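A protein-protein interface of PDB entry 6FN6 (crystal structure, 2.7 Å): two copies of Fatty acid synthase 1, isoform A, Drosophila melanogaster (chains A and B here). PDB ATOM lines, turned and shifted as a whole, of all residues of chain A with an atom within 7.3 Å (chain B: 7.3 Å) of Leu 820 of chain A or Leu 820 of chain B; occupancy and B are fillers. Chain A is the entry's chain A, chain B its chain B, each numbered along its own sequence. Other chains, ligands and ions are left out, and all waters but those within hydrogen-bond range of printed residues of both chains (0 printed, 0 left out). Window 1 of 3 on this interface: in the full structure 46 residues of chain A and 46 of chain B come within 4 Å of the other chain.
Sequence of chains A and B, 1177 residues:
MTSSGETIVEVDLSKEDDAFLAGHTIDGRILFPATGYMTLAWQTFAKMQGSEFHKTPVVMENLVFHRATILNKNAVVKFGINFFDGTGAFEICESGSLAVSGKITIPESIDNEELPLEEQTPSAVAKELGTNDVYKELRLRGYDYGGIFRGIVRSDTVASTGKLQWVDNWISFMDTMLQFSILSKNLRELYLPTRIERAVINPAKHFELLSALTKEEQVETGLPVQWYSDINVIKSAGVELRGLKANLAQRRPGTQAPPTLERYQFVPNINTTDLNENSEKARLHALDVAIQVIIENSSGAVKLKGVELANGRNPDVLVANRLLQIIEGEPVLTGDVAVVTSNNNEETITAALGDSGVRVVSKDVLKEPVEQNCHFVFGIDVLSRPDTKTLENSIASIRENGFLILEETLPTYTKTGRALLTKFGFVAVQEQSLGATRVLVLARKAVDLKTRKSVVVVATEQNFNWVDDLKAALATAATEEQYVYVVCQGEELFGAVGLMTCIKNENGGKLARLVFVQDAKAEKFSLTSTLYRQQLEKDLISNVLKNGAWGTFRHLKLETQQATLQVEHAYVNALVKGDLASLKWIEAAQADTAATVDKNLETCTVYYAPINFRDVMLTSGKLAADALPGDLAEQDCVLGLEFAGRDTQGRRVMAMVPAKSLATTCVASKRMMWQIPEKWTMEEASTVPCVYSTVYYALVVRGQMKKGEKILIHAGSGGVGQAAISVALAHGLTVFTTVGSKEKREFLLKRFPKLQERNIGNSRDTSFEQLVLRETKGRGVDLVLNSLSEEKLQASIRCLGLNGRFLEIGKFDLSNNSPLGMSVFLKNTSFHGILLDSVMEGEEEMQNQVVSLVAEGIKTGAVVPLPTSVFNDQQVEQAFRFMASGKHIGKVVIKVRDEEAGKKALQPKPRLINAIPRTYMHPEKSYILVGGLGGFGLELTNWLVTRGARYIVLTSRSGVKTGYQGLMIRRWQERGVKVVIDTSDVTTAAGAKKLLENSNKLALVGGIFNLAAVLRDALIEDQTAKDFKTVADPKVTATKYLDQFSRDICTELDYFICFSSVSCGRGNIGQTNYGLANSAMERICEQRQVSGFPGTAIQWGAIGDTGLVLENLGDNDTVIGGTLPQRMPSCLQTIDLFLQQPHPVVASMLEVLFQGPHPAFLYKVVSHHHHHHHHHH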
ATOM      1  N   LEU A 793      21.193 -20.185  13.124  1.00  0.00           N
ATOM      2  CA  LEU A 793      20.167 -21.012  13.754  1.00  0.00           C
ATOM      3  C   LEU A 793      18.852 -20.245  13.837  1.00  0.00           C
ATOM      4  O   LEU A 793      17.804 -20.751  13.441  1.00  0.00           O
ATOM      5  CB  LEU A 793      20.611 -21.459  15.151  1.00  0.00           C
ATOM      6  CG  LEU A 793      19.754 -22.531  15.840  1.00  0.00           C
ATOM      7  CD1 LEU A 793      20.588 -23.330  16.820  1.00  0.00           C
ATOM      8  CD2 LEU A 793      18.558 -21.933  16.567  1.00  0.00           C
ATOM      9  N   GLN A 794      18.913 -19.024  14.360  1.00  0.00           N
ATOM     10  CA  GLN A 794      17.729 -18.182  14.465  1.00  0.00           C
ATOM     11  C   GLN A 794      17.138 -17.925  13.079  1.00  0.00           C
ATOM     12  O   GLN A 794      15.922 -17.791  12.926  1.00  0.00           O
ATOM     13  CB  GLN A 794      18.059 -16.861  15.166  1.00  0.00           C
ATOM     14  CG  GLN A 794      17.997 -16.934  16.690  1.00  0.00           C
ATOM     15  CD  GLN A 794      16.574 -17.099  17.216  1.00  0.00           C
ATOM     16  OE1 GLN A 794      15.633 -17.288  16.445  1.00  0.00           O
ATOM     17  NE2 GLN A 794      16.414 -17.021  18.533  1.00  0.00           N
ATOM     18  N   ILE A 797      15.249 -20.938  12.191  1.00  0.00           N
ATOM     19  CA  ILE A 797      13.983 -20.930  12.911  1.00  0.00           C
ATOM     20  C   ILE A 797      12.938 -20.187  12.090  1.00  0.00           C
ATOM     21  O   ILE A 797      11.800 -20.638  11.956  1.00  0.00           O
ATOM     22  CB  ILE A 797      14.154 -20.303  14.313  1.00  0.00           C
ATOM     23  CG1 ILE A 797      14.943 -21.243  15.228  1.00  0.00           C
ATOM     24  CG2 ILE A 797      12.801 -19.943  14.928  1.00  0.00           C
ATOM     25  CD1 ILE A 797      14.189 -22.489  15.657  1.00  0.00           C
ATOM     26  N   PHE A 806      11.555 -28.651  14.349  1.00  0.00           N
ATOM     27  CA  PHE A 806      12.975 -28.329  14.296  1.00  0.00           C
ATOM     28  C   PHE A 806      13.806 -29.459  14.895  1.00  0.00           C
ATOM     29  O   PHE A 806      13.542 -29.921  16.004  1.00  0.00           O
ATOM     30  CB  PHE A 806      13.247 -27.022  15.039  1.00  0.00           C
ATOM     31  CG  PHE A 806      14.516 -26.337  14.624  1.00  0.00           C
ATOM     32  CD1 PHE A 806      15.722 -26.642  15.233  1.00  0.00           C
ATOM     33  CD2 PHE A 806      14.500 -25.376  13.627  1.00  0.00           C
ATOM     34  CE1 PHE A 806      16.887 -26.003  14.853  1.00  0.00           C
ATOM     35  CE2 PHE A 806      15.662 -24.735  13.243  1.00  0.00           C
ATOM     36  CZ  PHE A 806      16.857 -25.049  13.856  1.00  0.00           C
ATOM     37  N   ASN A 817      23.780 -22.589  26.075  1.00  0.00           N
ATOM     38  CA  ASN A 817      22.482 -22.266  26.656  1.00  0.00           C
ATOM     39  C   ASN A 817      21.943 -20.982  26.031  1.00  0.00           C
ATOM     40  O   ASN A 817      21.413 -20.116  26.727  1.00  0.00           O
ATOM     41  CB  ASN A 817      22.590 -22.117  28.175  1.00  0.00           C
ATOM     42  CG  ASN A 817      21.238 -21.953  28.843  1.00  0.00           C
ATOM     43  OD1 ASN A 817      20.289 -22.677  28.537  1.00  0.00           O
ATOM     44  ND2 ASN A 817      21.144 -20.999  29.763  1.00  0.00           N
ATOM     45  N   SER A 818      22.096 -20.860  24.715  1.00  0.00           N
ATOM     46  CA  SER A 818      21.629 -19.680  23.993  1.00  0.00           C
ATOM     47  C   SER A 818      20.129 -19.473  24.192  1.00  0.00           C
ATOM     48  O   SER A 818      19.389 -20.435  24.404  1.00  0.00           O
ATOM     49  CB  SER A 818      21.944 -19.802  22.503  1.00  0.00           C
ATOM     50  OG  SER A 818      23.338 -19.911  22.279  1.00  0.00           O
ATOM     51  N   PRO A 819      19.669 -18.215  24.119  1.00  0.00           N
ATOM     52  CA  PRO A 819      18.234 -17.978  24.288  1.00  0.00           C
ATOM     53  C   PRO A 819      17.449 -18.275  23.016  1.00  0.00           C
ATOM     54  O   PRO A 819      17.908 -17.953  21.921  1.00  0.00           O
ATOM     55  CB  PRO A 819      18.165 -16.490  24.643  1.00  0.00           C
ATOM     56  CG  PRO A 819      19.430 -15.882  24.086  1.00  0.00           C
ATOM     57  CD  PRO A 819      20.377 -16.993  23.700  1.00  0.00           C
ATOM     58  N   LEU A 820      16.284 -18.894  23.170  1.00  0.00           N
ATOM     59  CA  LEU A 820      15.425 -19.210  22.035  1.00  0.00           C
ATOM     60  C   LEU A 820      14.102 -18.467  22.143  1.00  0.00           C
ATOM     61  O   LEU A 820      13.363 -18.641  23.112  1.00  0.00           O
ATOM     62  CB  LEU A 820      15.169 -20.715  21.957  1.00  0.00           C
ATOM     63  CG  LEU A 820      14.249 -21.181  20.829  1.00  0.00           C
ATOM     64  CD1 LEU A 820      14.926 -20.987  19.479  1.00  0.00           C
ATOM     65  CD2 LEU A 820      13.843 -22.630  21.031  1.00  0.00           C
ATOM     66  N   GLY A 821      13.809 -17.639  21.145  1.00  0.00           N
ATOM     67  CA  GLY A 821      12.545 -16.929  21.097  1.00  0.00           C
ATOM     68  C   GLY A 821      11.385 -17.899  20.993  1.00  0.00           C
ATOM     69  O   GLY A 821      11.281 -18.651  20.028  1.00  0.00           O
ATOM     70  N   MET A 822      10.510 -17.879  21.992  1.00  0.00           N
ATOM     71  CA  MET A 822       9.427 -18.852  22.078  1.00  0.00           C
ATOM     72  C   MET A 822       8.223 -18.500  21.195  1.00  0.00           C
ATOM     73  O   MET A 822       7.211 -19.201  21.217  1.00  0.00           O
ATOM     74  CB  MET A 822       8.980 -19.003  23.534  1.00  0.00           C
ATOM     75  CG  MET A 822      10.014 -19.687  24.411  1.00  0.00           C
ATOM     76  SD  MET A 822       9.524 -19.847  26.140  1.00  0.00           S
ATOM     77  CE  MET A 822       8.154 -20.989  25.995  1.00  0.00           C
ATOM     78  N   SER A 823       8.323 -17.418  20.430  1.00  0.00           N
ATOM     79  CA  SER A 823       7.252 -17.048  19.509  1.00  0.00           C
ATOM     80  C   SER A 823       7.071 -18.137  18.453  1.00  0.00           C
ATOM     81  O   SER A 823       5.965 -18.359  17.960  1.00  0.00           O
ATOM     82  CB  SER A 823       7.544 -15.705  18.834  1.00  0.00           C
ATOM     83  OG  SER A 823       8.627 -15.806  17.927  1.00  0.00           O
ATOM     84  N   VAL A 824       8.170 -18.802  18.107  1.00  0.00           N
ATOM     85  CA  VAL A 824       8.159 -19.858  17.099  1.00  0.00           C
ATOM     86  C   VAL A 824       7.154 -20.952  17.438  1.00  0.00           C
ATOM     87  O   VAL A 824       6.639 -21.630  16.546  1.00  0.00           O
ATOM     88  CB  VAL A 824       9.567 -20.467  16.931  1.00  0.00           C
ATOM     89  CG1 VAL A 824      10.024 -21.123  18.228  1.00  0.00           C
ATOM     90  CG2 VAL A 824       9.584 -21.472  15.782  1.00  0.00           C
ATOM     91  N   PHE A 825       6.889 -21.132  18.727  1.00  0.00           N
ATOM     92  CA  PHE A 825       6.017 -22.208  19.180  1.00  0.00           C
ATOM     93  C   PHE A 825       4.536 -21.852  19.032  1.00  0.00           C
ATOM     94  O   PHE A 825       3.668 -22.712  19.188  1.00  0.00           O
ATOM     95  CB  PHE A 825       6.349 -22.573  20.628  1.00  0.00           C
ATOM     96  CG  PHE A 825       7.730 -23.148  20.800  1.00  0.00           C
ATOM     97  CD1 PHE A 825       8.069 -24.355  20.208  1.00  0.00           C
ATOM     98  CD2 PHE A 825       8.690 -22.482  21.546  1.00  0.00           C
ATOM     99  CE1 PHE A 825       9.340 -24.889  20.360  1.00  0.00           C
ATOM    100  CE2 PHE A 825       9.963 -23.012  21.701  1.00  0.00           C
ATOM    101  CZ  PHE A 825      10.287 -24.216  21.107  1.00  0.00           C
ATOM    102  N   PHE A 831      10.455 -28.299  18.942  1.00  0.00           N
ATOM    103  CA  PHE A 831      11.908 -28.230  18.902  1.00  0.00           C
ATOM    104  C   PHE A 831      12.473 -29.516  19.499  1.00  0.00           C
ATOM    105  O   PHE A 831      12.122 -29.891  20.616  1.00  0.00           O
ATOM    106  CB  PHE A 831      12.421 -27.007  19.660  1.00  0.00           C
ATOM    107  CG  PHE A 831      13.836 -26.637  19.319  1.00  0.00           C
ATOM    108  CD1 PHE A 831      14.902 -27.347  19.848  1.00  0.00           C
ATOM    109  CD2 PHE A 831      14.099 -25.580  18.465  1.00  0.00           C
ATOM    110  CE1 PHE A 831      16.200 -27.009  19.530  1.00  0.00           C
ATOM    111  CE2 PHE A 831      15.396 -25.236  18.146  1.00  0.00           C
ATOM    112  CZ  PHE A 831      16.447 -25.954  18.677  1.00  0.00           C
ATOM    113  N   LEU B 793       7.344 -21.202  34.618  1.00  0.00           N
ATOM    114  CA  LEU B 793       7.596 -21.972  33.406  1.00  0.00           C
ATOM    115  C   LEU B 793       9.037 -22.462  33.423  1.00  0.00           C
ATOM    116  O   LEU B 793       9.305 -23.639  33.195  1.00  0.00           O
ATOM    117  CB  LEU B 793       7.325 -21.128  32.154  1.00  0.00           C
ATOM    118  CG  LEU B 793       7.315 -21.858  30.803  1.00  0.00           C
ATOM    119  CD1 LEU B 793       6.433 -21.125  29.802  1.00  0.00           C
ATOM    120  CD2 LEU B 793       8.722 -22.018  30.233  1.00  0.00           C
ATOM    121  N   GLN B 794       9.957 -21.548  33.703  1.00  0.00           N
ATOM    122  CA  GLN B 794      11.373 -21.877  33.765  1.00  0.00           C
ATOM    123  C   GLN B 794      11.616 -22.965  34.811  1.00  0.00           C
ATOM    124  O   GLN B 794      12.484 -23.822  34.644  1.00  0.00           O
ATOM    125  CB  GLN B 794      12.189 -20.624  34.094  1.00  0.00           C
ATOM    126  CG  GLN B 794      12.501 -19.755  32.885  1.00  0.00           C
ATOM    127  CD  GLN B 794      12.851 -18.327  33.266  1.00  0.00           C
ATOM    128  OE1 GLN B 794      13.421 -18.075  34.328  1.00  0.00           O
ATOM    129  NE2 GLN B 794      12.500 -17.382  32.401  1.00  0.00           N
ATOM    130  N   ILE B 797      10.568 -26.359  33.401  1.00  0.00           N
ATOM    131  CA  ILE B 797      11.605 -26.879  32.514  1.00  0.00           C
ATOM    132  C   ILE B 797      12.627 -27.687  33.308  1.00  0.00           C
ATOM    133  O   ILE B 797      13.041 -28.768  32.886  1.00  0.00           O
ATOM    134  CB  ILE B 797      12.286 -25.730  31.730  1.00  0.00           C
ATOM    135  CG1 ILE B 797      11.346 -25.190  30.652  1.00  0.00           C
ATOM    136  CG2 ILE B 797      13.625 -26.169  31.131  1.00  0.00           C
ATOM    137  CD1 ILE B 797      11.131 -26.135  29.475  1.00  0.00           C
ATOM    138  N   PHE B 806       8.302 -31.583  26.917  1.00  0.00           N
ATOM    139  CA  PHE B 806       7.550 -30.473  27.485  1.00  0.00           C
ATOM    140  C   PHE B 806       6.371 -30.129  26.577  1.00  0.00           C
ATOM    141  O   PHE B 806       6.534 -29.974  25.368  1.00  0.00           O
ATOM    142  CB  PHE B 806       8.458 -29.256  27.678  1.00  0.00           C
ATOM    143  CG  PHE B 806       7.937 -28.261  28.676  1.00  0.00           C
ATOM    144  CD1 PHE B 806       7.149 -27.198  28.266  1.00  0.00           C
ATOM    145  CD2 PHE B 806       8.236 -28.388  30.022  1.00  0.00           C
ATOM    146  CE1 PHE B 806       6.668 -26.281  29.179  1.00  0.00           C
ATOM    147  CE2 PHE B 806       7.756 -27.473  30.941  1.00  0.00           C
ATOM    148  CZ  PHE B 806       6.972 -26.417  30.518  1.00  0.00           C
ATOM    149  N   ASN B 817       7.100 -13.803  23.381  1.00  0.00           N
ATOM    150  CA  ASN B 817       8.351 -14.271  22.789  1.00  0.00           C
ATOM    151  C   ASN B 817       9.438 -14.387  23.856  1.00  0.00           C
ATOM    152  O   ASN B 817      10.584 -13.986  23.639  1.00  0.00           O
ATOM    153  CB  ASN B 817       8.805 -13.330  21.666  1.00  0.00           C
ATOM    154  CG  ASN B 817      10.013 -13.862  20.907  1.00  0.00           C
ATOM    155  OD1 ASN B 817      10.066 -15.036  20.545  1.00  0.00           O
ATOM    156  ND2 ASN B 817      10.987 -12.993  20.660  1.00  0.00           N
ATOM    157  N   SER B 818       9.070 -14.924  25.015  1.00  0.00           N
ATOM    158  CA  SER B 818      10.025 -15.091  26.105  1.00  0.00           C
ATOM    159  C   SER B 818      11.198 -15.952  25.646  1.00  0.00           C
ATOM    160  O   SER B 818      11.027 -16.823  24.795  1.00  0.00           O
ATOM    161  CB  SER B 818       9.355 -15.728  27.320  1.00  0.00           C
ATOM    162  OG  SER B 818       8.295 -14.924  27.806  1.00  0.00           O
ATOM    163  N   PRO B 819      12.392 -15.723  26.218  1.00  0.00           N
ATOM    164  CA  PRO B 819      13.557 -16.521  25.827  1.00  0.00           C
ATOM    165  C   PRO B 819      13.610 -17.872  26.531  1.00  0.00           C
ATOM    166  O   PRO B 819      13.305 -17.948  27.721  1.00  0.00           O
ATOM    167  CB  PRO B 819      14.736 -15.642  26.244  1.00  0.00           C
ATOM    168  CG  PRO B 819      14.204 -14.743  27.333  1.00  0.00           C
ATOM    169  CD  PRO B 819      12.698 -14.838  27.353  1.00  0.00           C
ATOM    170  N   LEU B 820      13.987 -18.916  25.798  1.00  0.00           N
ATOM    171  CA  LEU B 820      14.112 -20.257  26.360  1.00  0.00           C
ATOM    172  C   LEU B 820      15.553 -20.754  26.279  1.00  0.00           C
ATOM    173  O   LEU B 820      16.119 -20.862  25.191  1.00  0.00           O
ATOM    174  CB  LEU B 820      13.189 -21.229  25.629  1.00  0.00           C
ATOM    175  CG  LEU B 820      13.251 -22.688  26.084  1.00  0.00           C
ATOM    176  CD1 LEU B 820      12.686 -22.838  27.485  1.00  0.00           C
ATOM    177  CD2 LEU B 820      12.506 -23.574  25.102  1.00  0.00           C
ATOM    178  N   GLY B 821      16.138 -21.063  27.434  1.00  0.00           N
ATOM    179  CA  GLY B 821      17.485 -21.604  27.485  1.00  0.00           C
ATOM    180  C   GLY B 821      17.570 -22.939  26.770  1.00  0.00           C
ATOM    181  O   GLY B 821      16.894 -23.897  27.145  1.00  0.00           O
ATOM    182  N   MET B 822      18.400 -23.007  25.735  1.00  0.00           N
ATOM    183  CA  MET B 822      18.455 -24.196  24.892  1.00  0.00           C
ATOM    184  C   MET B 822      19.286 -25.321  25.510  1.00  0.00           C
ATOM    185  O   MET B 822      19.425 -26.389  24.916  1.00  0.00           O
ATOM    186  CB  MET B 822      19.020 -23.835  23.516  1.00  0.00           C
ATOM    187  CG  MET B 822      18.085 -22.970  22.679  1.00  0.00           C
ATOM    188  SD  MET B 822      18.766 -22.511  21.074  1.00  0.00           S
ATOM    189  CE  MET B 822      18.837 -24.103  20.273  1.00  0.00           C
ATOM    190  N   SER B 823      19.814 -25.091  26.708  1.00  0.00           N
ATOM    191  CA  SER B 823      20.585 -26.111  27.411  1.00  0.00           C
ATOM    192  C   SER B 823      19.719 -27.327  27.716  1.00  0.00           C
ATOM    193  O   SER B 823      20.202 -28.458  27.740  1.00  0.00           O
ATOM    194  CB  SER B 823      21.167 -25.545  28.705  1.00  0.00           C
ATOM    195  OG  SER B 823      20.140 -25.273  29.642  1.00  0.00           O
ATOM    196  N   VAL B 824      18.435 -27.080  27.945  1.00  0.00           N
ATOM    197  CA  VAL B 824      17.478 -28.136  28.254  1.00  0.00           C
ATOM    198  C   VAL B 824      17.470 -29.217  27.175  1.00  0.00           C
ATOM    199  O   VAL B 824      17.135 -30.371  27.447  1.00  0.00           O
ATOM    200  CB  VAL B 824      16.064 -27.551  28.440  1.00  0.00           C
ATOM    201  CG1 VAL B 824      15.577 -26.896  27.149  1.00  0.00           C
ATOM    202  CG2 VAL B 824      15.094 -28.630  28.900  1.00  0.00           C
ATOM    203  N   PHE B 825      17.830 -28.843  25.951  1.00  0.00           N
ATOM    204  CA  PHE B 825      17.771 -29.774  24.831  1.00  0.00           C
ATOM    205  C   PHE B 825      18.976 -30.717  24.813  1.00  0.00           C
ATOM    206  O   PHE B 825      18.986 -31.697  24.068  1.00  0.00           O
ATOM    207  CB  PHE B 825      17.680 -29.008  23.509  1.00  0.00           C
ATOM    208  CG  PHE B 825      16.433 -28.185  23.376  1.00  0.00           C
ATOM    209  CD1 PHE B 825      15.186 -28.788  23.372  1.00  0.00           C
ATOM    210  CD2 PHE B 825      16.507 -26.809  23.242  1.00  0.00           C
ATOM    211  CE1 PHE B 825      14.036 -28.033  23.254  1.00  0.00           C
ATOM    212  CE2 PHE B 825      15.360 -26.049  23.119  1.00  0.00           C
ATOM    213  CZ  PHE B 825      14.121 -26.663  23.124  1.00  0.00           C
ATOM    214  N   PHE B 831      10.387 -29.727  23.007  1.00  0.00           N
ATOM    215  CA  PHE B 831       9.434 -28.700  23.415  1.00  0.00           C
ATOM    216  C   PHE B 831       8.303 -28.639  22.393  1.00  0.00           C
ATOM    217  O   PHE B 831       8.546 -28.475  21.199  1.00  0.00           O
ATOM    218  CB  PHE B 831      10.114 -27.336  23.546  1.00  0.00           C
ATOM    219  CG  PHE B 831       9.304 -26.330  24.317  1.00  0.00           C
ATOM    220  CD1 PHE B 831       8.234 -25.678  23.723  1.00  0.00           C
ATOM    221  CD2 PHE B 831       9.609 -26.043  25.637  1.00  0.00           C
ATOM    222  CE1 PHE B 831       7.486 -24.755  24.428  1.00  0.00           C
ATOM    223  CE2 PHE B 831       8.864 -25.120  26.348  1.00  0.00           C
ATOM    224  CZ  PHE B 831       7.799 -24.477  25.743  1.00  0.00           C
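The backbone NH (N) of Phe 831 of chain B sits at hydrogen-bond distance from the backbone carbonyl oxygen (O) of Phe 831 of chain A, at 3.0 Å. O of Ser 818 of chain B lies close to O of Leu 820 of chain A (3.4 Å). The side-chain hydroxyl (OG) of Ser 823 of chain B lies within hydrogen-bond range of the side-chain amide oxygen (OD1) of Asn 817 of chain A. The side-chain amide oxygen of Asn 817 of chain A sits at hydrogen-bond distance from the backbone NH of Met 822 of chain B. O of Ser 818 of chain A sits close to O of Leu 820 of chain B (3.4 Å). The backbone carbonyl oxygen (O) of Ser 818 of chain A lies within hydrogen-bond range of the backbone NH (N) of Met 822 of chain B (3.1 Å). N of Leu 820 of chain B is in hydrogen-bond range of O of Leu 820 of chain A, at 2.8 Å. The side-chain amide oxygen (OD1) of Asn 817 of chain B lies within hydrogen-bond range of the backbone NH (N) of Ser 823 of chain A. N of Met 822 of chain A lies within hydrogen-bond range of OD1 of Asn 817 of chain B (3.2 Å). The backbone NH of Met 822 of chain A sits at hydrogen-bond distance from the backbone carbonyl oxygen of Ser 818 of chain B, 3.0 Å away.
Among the printed residues, merely in contact across the chains: Leu 793 of chain A with Met 822 of chain B, Asn 817 of chain A with Gly 821 of chain B, Ser 818 of chain A with Gly 821 of chain B, Pro 819 of chain A with Pro 819 of chain B, Pro 819 of chain A with Leu 820 of chain B, Leu 820 of chain A with Pro 819 of chain B, Leu 820 of chain A with Met 822 of chain B, Gly 821 of chain A with Asn 817 of chain B, Gly 821 of chain A with Ser 818 of chain B, Met 822 of chain A with Leu 820 of chain B, Met 822 of chain A with Phe 831 of chain B, Phe 825 of chain A with Phe 831 of chain B, Phe 831 of chain A with Met 822 of chain B and Phe 831 of chain A with Phe 825 of chain B.
Leu 820 of chain A touches just these residues of chain B: Ser 818 (3.4 Å), Pro 819 (3.5 Å), Leu 820 (2.8 Å) and Met 822 (3.8 Å). Of the printed residues of chain B, Phe 831 of chain A touches Met 822, Phe 825 and Phe 831. Of the printed residues of chain A, Ser 823 of chain B touches Asn 817 (2.8 Å). Printed residues of chain B within 4 Å of Ser 823 of chain A: Asn 817. Printed residues of chain A within 4 Å of Phe 825 of chain B: Phe 831. Of the printed residues of chain B, Leu 793 of chain A touches Met 822.
Of the 14 printed residues of chain A, 10 touch a printed residue of chain B. Hydrophobic or aromatic side chains of chain A within 4 Å of the printed part of chain B: Leu 793, Pro 819, Leu 820, Met 822, Phe 825 and Phe 831. Of the 14 printed residues of chain B, 9 touch a printed residue of chain A. Hydrophobic or aromatic side chains of chain B that line the printed part of chain A: Pro 819, Leu 820, Met 822, Phe 825 and Phe 831. Among the printed residues, 24 pairs touch across the chains.
Leu 793 of chain A touches Met 822 of chain B, but with the chains exchanged Met 822 of chain A does not touch Leu 793 of chain B (4.2 Å). Asn 817 of chain A touches Gly 821 of chain B, and with the chains exchanged Gly 821 of chain A touches Asn 817 of chain B. Leu 820 of chain A touches Met 822 of chain B, and with the chains exchanged Met 822 of chain A touches Leu 820 of chain B. Phe 831 of chain A touches its own counterpart, Phe 831 of chain B. 14 positions are printed for both chains. Of the 24 pairs that touch across the chains among the printed residues, 23 have their exchanged pair printed and touching as well.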
